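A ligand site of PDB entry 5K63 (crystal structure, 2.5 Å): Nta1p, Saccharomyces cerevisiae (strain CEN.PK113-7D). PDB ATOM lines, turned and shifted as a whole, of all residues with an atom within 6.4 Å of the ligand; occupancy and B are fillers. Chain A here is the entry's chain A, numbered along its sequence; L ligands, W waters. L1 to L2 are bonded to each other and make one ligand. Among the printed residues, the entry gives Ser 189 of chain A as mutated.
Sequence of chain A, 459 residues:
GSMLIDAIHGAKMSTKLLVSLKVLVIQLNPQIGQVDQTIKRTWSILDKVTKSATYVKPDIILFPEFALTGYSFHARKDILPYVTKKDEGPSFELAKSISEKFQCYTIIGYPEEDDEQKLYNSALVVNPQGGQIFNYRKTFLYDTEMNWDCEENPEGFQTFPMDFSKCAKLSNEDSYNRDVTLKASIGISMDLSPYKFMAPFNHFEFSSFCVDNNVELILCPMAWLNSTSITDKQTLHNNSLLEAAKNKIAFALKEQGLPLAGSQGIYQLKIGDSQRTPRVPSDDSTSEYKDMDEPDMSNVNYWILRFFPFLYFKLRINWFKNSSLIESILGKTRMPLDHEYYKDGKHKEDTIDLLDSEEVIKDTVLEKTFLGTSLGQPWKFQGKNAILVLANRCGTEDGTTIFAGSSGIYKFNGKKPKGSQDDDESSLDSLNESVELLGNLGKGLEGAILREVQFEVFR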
ATOM      1  N   GLU A  65      -5.183   5.571  26.131  1.00  0.00           N
ATOM      2  CA  GLU A  65      -5.783   6.894  26.229  1.00  0.00           C
ATOM      3  C   GLU A  65      -4.915   7.762  27.147  1.00  0.00           C
ATOM      4  O   GLU A  65      -4.477   7.297  28.207  1.00  0.00           O
ATOM      5  CB  GLU A  65      -7.216   6.782  26.742  1.00  0.00           C
ATOM      6  CG  GLU A  65      -7.944   8.090  26.953  1.00  0.00           C
ATOM      7  CD  GLU A  65      -9.403   7.872  27.362  1.00  0.00           C
ATOM      8  OE1 GLU A  65      -9.791   6.692  27.504  1.00  0.00           O
ATOM      9  OE2 GLU A  65     -10.138   8.873  27.525  1.00  0.00           O
ATOM     10  N   TYR A  71      -4.489  10.821  33.539  1.00  0.00           N
ATOM     11  CA  TYR A  71      -5.867  10.907  33.060  1.00  0.00           C
ATOM     12  C   TYR A  71      -6.810  11.773  33.890  1.00  0.00           C
ATOM     13  O   TYR A  71      -7.687  12.451  33.349  1.00  0.00           O
ATOM     14  CB  TYR A  71      -6.474   9.503  32.945  1.00  0.00           C
ATOM     15  CG  TYR A  71      -7.893   9.507  32.446  1.00  0.00           C
ATOM     16  CD1 TYR A  71      -8.186   9.840  31.135  1.00  0.00           C
ATOM     17  CD2 TYR A  71      -8.958   9.194  33.287  1.00  0.00           C
ATOM     18  CE1 TYR A  71      -9.471   9.866  30.667  1.00  0.00           C
ATOM     19  CE2 TYR A  71     -10.264   9.215  32.831  1.00  0.00           C
ATOM     20  CZ  TYR A  71     -10.517   9.541  31.510  1.00  0.00           C
ATOM     21  OH  TYR A  71     -11.802   9.567  31.042  1.00  0.00           O
ATOM     22  N   LYS A 138     -12.423  11.787  20.884  1.00  0.00           N
ATOM     23  CA  LYS A 138     -13.341  10.991  21.683  1.00  0.00           C
ATOM     24  C   LYS A 138     -14.777  11.489  21.468  1.00  0.00           C
ATOM     25  O   LYS A 138     -15.056  12.692  21.501  1.00  0.00           O
ATOM     26  CB  LYS A 138     -12.956  11.045  23.171  1.00  0.00           C
ATOM     27  CG  LYS A 138     -13.581   9.958  24.017  1.00  0.00           C
ATOM     28  CD  LYS A 138     -13.131  10.064  25.465  1.00  0.00           C
ATOM     29  CE  LYS A 138     -13.624   8.889  26.301  1.00  0.00           C
ATOM     30  NZ  LYS A 138     -13.089   8.889  27.702  1.00  0.00           N
ATOM     31  N   PHE A 140     -17.921   9.693  22.816  1.00  0.00           N
ATOM     32  CA  PHE A 140     -18.684   9.577  24.069  1.00  0.00           C
ATOM     33  C   PHE A 140     -17.786   9.951  25.246  1.00  0.00           C
ATOM     34  O   PHE A 140     -16.769   9.299  25.493  1.00  0.00           O
ATOM     35  CB  PHE A 140     -19.211   8.156  24.246  1.00  0.00           C
ATOM     36  CG  PHE A 140     -20.328   7.792  23.310  1.00  0.00           C
ATOM     37  CD1 PHE A 140     -20.826   8.701  22.391  1.00  0.00           C
ATOM     38  CD2 PHE A 140     -20.894   6.518  23.350  1.00  0.00           C
ATOM     39  CE1 PHE A 140     -21.863   8.365  21.521  1.00  0.00           C
ATOM     40  CE2 PHE A 140     -21.934   6.168  22.477  1.00  0.00           C
ATOM     41  CZ  PHE A 140     -22.416   7.095  21.560  1.00  0.00           C
ATOM     42  N   LEU A 141     -18.130  11.011  25.963  1.00  0.00           N
ATOM     43  CA  LEU A 141     -17.282  11.474  27.051  1.00  0.00           C
ATOM     44  C   LEU A 141     -17.646  10.826  28.399  1.00  0.00           C
ATOM     45  O   LEU A 141     -18.782  10.433  28.642  1.00  0.00           O
ATOM     46  CB  LEU A 141     -17.338  13.001  27.161  1.00  0.00           C
ATOM     47  CG  LEU A 141     -17.061  13.782  25.877  1.00  0.00           C
ATOM     48  CD1 LEU A 141     -17.095  15.286  26.123  1.00  0.00           C
ATOM     49  CD2 LEU A 141     -15.737  13.350  25.250  1.00  0.00           C
ATOM     50  N   TYR A 142     -16.640  10.699  29.255  1.00  0.00           N
ATOM     51  CA  TYR A 142     -16.826  10.194  30.610  1.00  0.00           C
ATOM     52  C   TYR A 142     -16.831  11.398  31.553  1.00  0.00           C
ATOM     53  O   TYR A 142     -16.446  12.496  31.157  1.00  0.00           O
ATOM     54  CB  TYR A 142     -15.730   9.175  30.939  1.00  0.00           C
ATOM     55  CG  TYR A 142     -15.752   8.597  32.320  1.00  0.00           C
ATOM     56  CD1 TYR A 142     -16.795   7.773  32.731  1.00  0.00           C
ATOM     57  CD2 TYR A 142     -14.703   8.824  33.207  1.00  0.00           C
ATOM     58  CE1 TYR A 142     -16.820   7.224  34.006  1.00  0.00           C
ATOM     59  CE2 TYR A 142     -14.713   8.279  34.482  1.00  0.00           C
ATOM     60  CZ  TYR A 142     -15.771   7.478  34.869  1.00  0.00           C
ATOM     61  OH  TYR A 142     -15.785   6.943  36.135  1.00  0.00           O
ATOM     62  N   ASP A 143     -17.258  11.205  32.802  1.00  0.00           N
ATOM     63  CA  ASP A 143     -17.348  12.305  33.770  1.00  0.00           C
ATOM     64  C   ASP A 143     -16.059  13.129  33.899  1.00  0.00           C
ATOM     65  O   ASP A 143     -16.109  14.358  33.945  1.00  0.00           O
ATOM     66  CB  ASP A 143     -17.729  11.759  35.148  1.00  0.00           C
ATOM     67  CG  ASP A 143     -19.076  11.073  35.141  1.00  0.00           C
ATOM     68  OD1 ASP A 143     -19.487  10.564  34.079  1.00  0.00           O
ATOM     69  OD2 ASP A 143     -19.711  11.043  36.220  1.00  0.00           O
ATOM     70  N   GLU A 145     -13.809  13.866  31.777  1.00  0.00           N
ATOM     71  CA  GLU A 145     -13.681  14.832  30.696  1.00  0.00           C
ATOM     72  C   GLU A 145     -14.504  16.090  30.938  1.00  0.00           C
ATOM     73  O   GLU A 145     -14.146  17.177  30.476  1.00  0.00           O
ATOM     74  CB  GLU A 145     -14.087  14.192  29.357  1.00  0.00           C
ATOM     75  CG  GLU A 145     -12.955  13.434  28.662  1.00  0.00           C
ATOM     76  CD  GLU A 145     -12.914  11.978  29.064  1.00  0.00           C
ATOM     77  OE1 GLU A 145     -13.950  11.293  28.913  1.00  0.00           O
ATOM     78  OE2 GLU A 145     -11.848  11.523  29.533  1.00  0.00           O
ATOM     79  N   ILE A 188     -12.070   5.509  21.551  1.00  0.00           N
ATOM     80  CA  ILE A 188     -11.444   5.761  22.840  1.00  0.00           C
ATOM     81  C   ILE A 188     -12.393   5.390  23.991  1.00  0.00           C
ATOM     82  O   ILE A 188     -13.502   5.912  24.061  1.00  0.00           O
ATOM     83  CB  ILE A 188     -11.004   7.247  22.960  1.00  0.00           C
ATOM     84  CG1 ILE A 188     -10.027   7.599  21.832  1.00  0.00           C
ATOM     85  CG2 ILE A 188     -10.381   7.530  24.315  1.00  0.00           C
ATOM     86  CD1 ILE A 188      -9.621   9.076  21.776  1.00  0.00           C
ATOM     87  N   SER A 189     -11.935   4.492  24.863  1.00  0.00           N
ATOM     88  CA  SER A 189     -12.657   3.966  26.049  1.00  0.00           C
ATOM     89  C   SER A 189     -14.193   4.104  26.090  1.00  0.00           C
ATOM     90  O   SER A 189     -14.907   3.200  25.662  1.00  0.00           O
ATOM     91  CB  SER A 189     -12.074   4.610  27.312  1.00  0.00           C
ATOM     92  OG  SER A 189     -12.382   5.993  27.397  1.00  0.00           O
ATOM     93  N   MET A 190     -14.694   5.214  26.627  1.00  0.00           N
ATOM     94  CA  MET A 190     -16.134   5.447  26.788  1.00  0.00           C
ATOM     95  C   MET A 190     -16.962   5.318  25.486  1.00  0.00           C
ATOM     96  O   MET A 190     -18.173   5.158  25.535  1.00  0.00           O
ATOM     97  CB  MET A 190     -16.365   6.849  27.404  1.00  0.00           C
ATOM     98  CG  MET A 190     -17.825   7.194  27.691  1.00  0.00           C
ATOM     99  SD  MET A 190     -18.479   6.340  29.151  1.00  0.00           S
ATOM    100  CE  MET A 190     -20.222   6.776  29.080  1.00  0.00           C
ATOM    101  N   ASP A 191     -16.295   5.385  24.330  1.00  0.00           N
ATOM    102  CA  ASP A 191     -16.973   5.179  23.055  1.00  0.00           C
ATOM    103  C   ASP A 191     -17.672   3.834  23.012  1.00  0.00           C
ATOM    104  O   ASP A 191     -18.659   3.668  22.305  1.00  0.00           O
ATOM    105  CB  ASP A 191     -15.970   5.267  21.892  1.00  0.00           C
ATOM    106  CG  ASP A 191     -15.547   6.687  21.580  1.00  0.00           C
ATOM    107  OD1 ASP A 191     -16.273   7.637  21.951  1.00  0.00           O
ATOM    108  OD2 ASP A 191     -14.488   6.878  20.950  1.00  0.00           O
ATOM    109  N   SER A 193     -19.083   2.332  25.605  1.00  0.00           N
ATOM    110  CA  SER A 193     -20.211   2.333  26.535  1.00  0.00           C
ATOM    111  C   SER A 193     -21.473   2.846  25.856  1.00  0.00           C
ATOM    112  O   SER A 193     -21.390   3.512  24.820  1.00  0.00           O
ATOM    113  CB  SER A 193     -19.914   3.199  27.758  1.00  0.00           C
ATOM    114  OG  SER A 193     -18.791   2.705  28.463  1.00  0.00           O
ATOM    115  N   PHE A 197     -24.058   6.475  29.611  1.00  0.00           N
ATOM    116  CA  PHE A 197     -24.533   5.404  30.499  1.00  0.00           C
ATOM    117  C   PHE A 197     -26.062   5.453  30.685  1.00  0.00           C
ATOM    118  O   PHE A 197     -26.598   4.740  31.517  1.00  0.00           O
ATOM    119  CB  PHE A 197     -23.863   5.474  31.875  1.00  0.00           C
ATOM    120  CG  PHE A 197     -22.371   5.238  31.853  1.00  0.00           C
ATOM    121  CD1 PHE A 197     -21.839   4.035  31.418  1.00  0.00           C
ATOM    122  CD2 PHE A 197     -21.502   6.216  32.327  1.00  0.00           C
ATOM    123  CE1 PHE A 197     -20.483   3.807  31.406  1.00  0.00           C
ATOM    124  CE2 PHE A 197     -20.131   5.988  32.332  1.00  0.00           C
ATOM    125  CZ  PHE A 197     -19.620   4.781  31.867  1.00  0.00           C
ATOM    126  N   MET A 222      -7.401   3.120  25.708  1.00  0.00           N
ATOM    127  CA  MET A 222      -8.328   3.192  26.834  1.00  0.00           C
ATOM    128  C   MET A 222      -7.706   3.617  28.148  1.00  0.00           C
ATOM    129  O   MET A 222      -6.517   3.405  28.400  1.00  0.00           O
ATOM    130  CB  MET A 222      -8.979   1.835  27.057  1.00  0.00           C
ATOM    131  CG  MET A 222      -9.968   1.419  26.013  1.00  0.00           C
ATOM    132  SD  MET A 222     -10.792  -0.071  26.587  1.00  0.00           S
ATOM    133  CE  MET A 222     -11.639  -0.538  25.072  1.00  0.00           C
ATOM    134  N   ALA A 223      -8.526   4.214  29.001  1.00  0.00           N
ATOM    135  CA  ALA A 223      -8.198   4.379  30.404  1.00  0.00           C
ATOM    136  C   ALA A 223      -9.360   3.813  31.221  1.00  0.00           C
ATOM    137  O   ALA A 223     -10.060   4.545  31.922  1.00  0.00           O
ATOM    138  CB  ALA A 223      -7.947   5.827  30.748  1.00  0.00           C
ATOM    139  N   TRP A 224      -9.575   2.507  31.087  1.00  0.00           N
ATOM    140  CA  TRP A 224     -10.775   1.847  31.597  1.00  0.00           C
ATOM    141  C   TRP A 224     -10.613   1.368  33.052  1.00  0.00           C
ATOM    142  O   TRP A 224      -9.557   0.873  33.430  1.00  0.00           O
ATOM    143  CB  TRP A 224     -11.121   0.671  30.696  1.00  0.00           C
ATOM    144  CG  TRP A 224     -12.515   0.155  30.854  1.00  0.00           C
ATOM    145  CD1 TRP A 224     -12.947  -0.743  31.792  1.00  0.00           C
ATOM    146  CD2 TRP A 224     -13.651   0.459  30.038  1.00  0.00           C
ATOM    147  NE1 TRP A 224     -14.286  -0.991  31.613  1.00  0.00           N
ATOM    148  CE2 TRP A 224     -14.740  -0.270  30.544  1.00  0.00           C
ATOM    149  CE3 TRP A 224     -13.849   1.287  28.921  1.00  0.00           C
ATOM    150  CZ2 TRP A 224     -16.017  -0.198  29.984  1.00  0.00           C
ATOM    151  CZ3 TRP A 224     -15.111   1.356  28.354  1.00  0.00           C
ATOM    152  CH2 TRP A 224     -16.182   0.618  28.886  1.00  0.00           C
ATOM    153  N   LEU A 225     -11.667   1.535  33.847  1.00  0.00           N
ATOM    154  CA  LEU A 225     -11.622   1.235  35.276  1.00  0.00           C
ATOM    155  C   LEU A 225     -11.863  -0.221  35.669  1.00  0.00           C
ATOM    156  O   LEU A 225     -12.735  -0.909  35.121  1.00  0.00           O
ATOM    157  CB  LEU A 225     -12.637   2.094  36.038  1.00  0.00           C
ATOM    158  CG  LEU A 225     -12.153   3.487  36.426  1.00  0.00           C
ATOM    159  CD1 LEU A 225     -11.606   4.189  35.189  1.00  0.00           C
ATOM    160  CD2 LEU A 225     -13.308   4.272  37.052  1.00  0.00           C
ATOM    161  N   ASN A 226     -11.080  -0.673  36.637  1.00  0.00           N
ATOM    162  CA  ASN A 226     -11.386  -1.876  37.401  1.00  0.00           C
ATOM    163  C   ASN A 226     -12.523  -1.542  38.379  1.00  0.00           C
ATOM    164  O   ASN A 226     -12.593  -0.414  38.885  1.00  0.00           O
ATOM    165  CB  ASN A 226     -10.131  -2.367  38.127  1.00  0.00           C
ATOM    166  CG  ASN A 226     -10.421  -3.504  39.094  1.00  0.00           C
ATOM    167  OD1 ASN A 226     -10.808  -3.263  40.237  1.00  0.00           O
ATOM    168  ND2 ASN A 226     -10.220  -4.741  38.651  1.00  0.00           N
ATOM    169  N   ASN A 299     -13.428  -7.430  33.175  1.00  0.00           N
ATOM    170  CA  ASN A 299     -13.364  -6.376  32.177  1.00  0.00           C
ATOM    171  C   ASN A 299     -13.221  -6.922  30.772  1.00  0.00           C
ATOM    172  O   ASN A 299     -13.808  -6.386  29.827  1.00  0.00           O
ATOM    173  CB  ASN A 299     -12.234  -5.403  32.484  1.00  0.00           C
ATOM    174  CG  ASN A 299     -12.699  -4.243  33.325  1.00  0.00           C
ATOM    175  OD1 ASN A 299     -12.044  -3.852  34.286  1.00  0.00           O
ATOM    176  ND2 ASN A 299     -13.851  -3.679  32.969  1.00  0.00           N
ATOM    177  N   TYR A 302     -16.523  -8.044  29.637  1.00  0.00           N
ATOM    178  CA  TYR A 302     -17.357  -6.895  29.389  1.00  0.00           C
ATOM    179  C   TYR A 302     -17.031  -6.200  28.071  1.00  0.00           C
ATOM    180  O   TYR A 302     -17.931  -5.844  27.315  1.00  0.00           O
ATOM    181  CB  TYR A 302     -17.240  -5.884  30.531  1.00  0.00           C
ATOM    182  CG  TYR A 302     -18.161  -4.718  30.340  1.00  0.00           C
ATOM    183  CD1 TYR A 302     -19.499  -4.804  30.722  1.00  0.00           C
ATOM    184  CD2 TYR A 302     -17.730  -3.533  29.746  1.00  0.00           C
ATOM    185  CE1 TYR A 302     -20.365  -3.741  30.540  1.00  0.00           C
ATOM    186  CE2 TYR A 302     -18.588  -2.473  29.570  1.00  0.00           C
ATOM    187  CZ  TYR A 302     -19.904  -2.581  29.963  1.00  0.00           C
ATOM    188  OH  TYR A 302     -20.771  -1.536  29.796  1.00  0.00           O
ATOM    189  N   PHE A 403      -7.228   1.658  37.259  1.00  0.00           N
ATOM    190  CA  PHE A 403      -7.382   1.228  35.876  1.00  0.00           C
ATOM    191  C   PHE A 403      -7.093  -0.264  35.757  1.00  0.00           C
ATOM    192  O   PHE A 403      -6.280  -0.809  36.490  1.00  0.00           O
ATOM    193  CB  PHE A 403      -6.505   2.061  34.940  1.00  0.00           C
ATOM    194  CG  PHE A 403      -6.724   3.540  35.075  1.00  0.00           C
ATOM    195  CD1 PHE A 403      -7.795   4.149  34.433  1.00  0.00           C
ATOM    196  CD2 PHE A 403      -5.894   4.314  35.875  1.00  0.00           C
ATOM    197  CE1 PHE A 403      -8.018   5.504  34.566  1.00  0.00           C
ATOM    198  CE2 PHE A 403      -6.118   5.669  36.008  1.00  0.00           C
ATOM    199  CZ  PHE A 403      -7.182   6.259  35.343  1.00  0.00           C
HETATM  200  N1  LIG L   1     -15.423   4.273  30.109  1.00  0.00           N
HETATM  201  C1  LIG L   1     -14.284   4.078  31.007  1.00  0.00           C
HETATM  202  C2  LIG L   1     -14.627   3.131  32.160  1.00  0.00           C
HETATM  203  O1  LIG L   1     -13.762   2.749  32.942  1.00  0.00           O
HETATM  204  C3  LIG L   1     -13.810   5.434  31.559  1.00  0.00           C
HETATM  205  C4  LIG L   1     -13.216   6.340  30.469  1.00  0.00           C
HETATM  206  O2  LIG L   1     -13.943   6.963  29.693  1.00  0.00           O
HETATM  207  N2  LIG L   1     -11.892   6.421  30.425  1.00  0.00           N
HETATM  208  N1  LG2 L   2     -15.894   2.753  32.261  1.00  0.00           N
HETATM  209  C1  LG2 L   2     -16.326   1.878  33.341  1.00  0.00           C
HETATM  210  C2  LG2 L   2     -17.783   1.489  33.264  1.00  0.00           C
HETATM  211  O1  LG2 L   2     -18.120   0.378  32.849  1.00  0.00           O
HETATM  212  O   HOH W   1     -19.792   1.004  29.938  1.00  0.00           O
HETATM  213  O   HOH W   2     -17.862  -2.689  33.337  1.00  0.00           O
HETATM  214  O   HOH W   3     -17.148   3.438  35.493  1.00  0.00           O
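An oxygen (O1) of LIG L1 sits at hydrogen-bond distance from the backbone NH of Leu 225. NZ of Lys 138 lies within hydrogen-bond range of O2 of LIG L1, 2.9 Å away. The side-chain hydroxyl (OG) of Ser 189 sits at hydrogen-bond distance from an oxygen (O2) of LIG L1, at 2.9 Å. The backbone carbonyl oxygen (O) of Ala 223 is in hydrogen-bond range of a nitrogen (N2) of LIG L1 (3.0 Å). The side-chain hydroxyl (OH) of Tyr 71 is in hydrogen-bond range of a nitrogen (N2) of LIG L1.
OD1 of Asn 299 sits close to O of Leu 225 (3.1 Å). The side-chain amino group of Lys 138 lies within hydrogen-bond range of the side-chain hydroxyl of Ser 189 (3.0 Å). OG of Ser 189 lies within hydrogen-bond range of OE1 of Glu 65 (2.7 Å). The backbone NH of Ala 223 is in hydrogen-bond range of the side-chain carboxylate of Glu 65. The backbone NH (N) of Tyr 142 is in hydrogen-bond range of the side-chain carboxylate (OE1) of Glu 145, 2.8 Å away. The side-chain hydroxyl (OH) of Tyr 71 is in hydrogen-bond range of the side-chain carboxylate (OE2) of Glu 145, 2.5 Å away. OG of Ser 193 is in hydrogen-bond range of SD of Met 190, 3.7 Å away. The indole nitrogen (NE1) of Trp 224 lies close to the side-chain amide nitrogen (ND2) of Asn 299 (3.0 Å).
OE1 of Glu 65 touches N2 of LIG L1, at 3.6 Å. CB of Tyr 142 touches O2 of LIG L1 (3.1 Å). Met 190 touches the ligand. CA of Trp 224 touches O1 of LIG L1, 3.4 Å away. Hydrophobic or aromatic side chains that line the ligand: Tyr 71, Tyr 142, Met 190, Trp 224 and Leu 225. Within 4 Å of the ligand: Glu 65, Tyr 71, Lys 138, Tyr 142, Ser 189, Met 190, Ala 223, Trp 224 and Leu 225.
Water W1 lies within hydrogen-bond range of the side-chain hydroxyl (OG) of Ser 193 (2.5 Å), the side-chain hydroxyl (OH) of Tyr 302 (2.7 Å) and an oxygen (O1) of LG2 L2 (3.4 Å).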
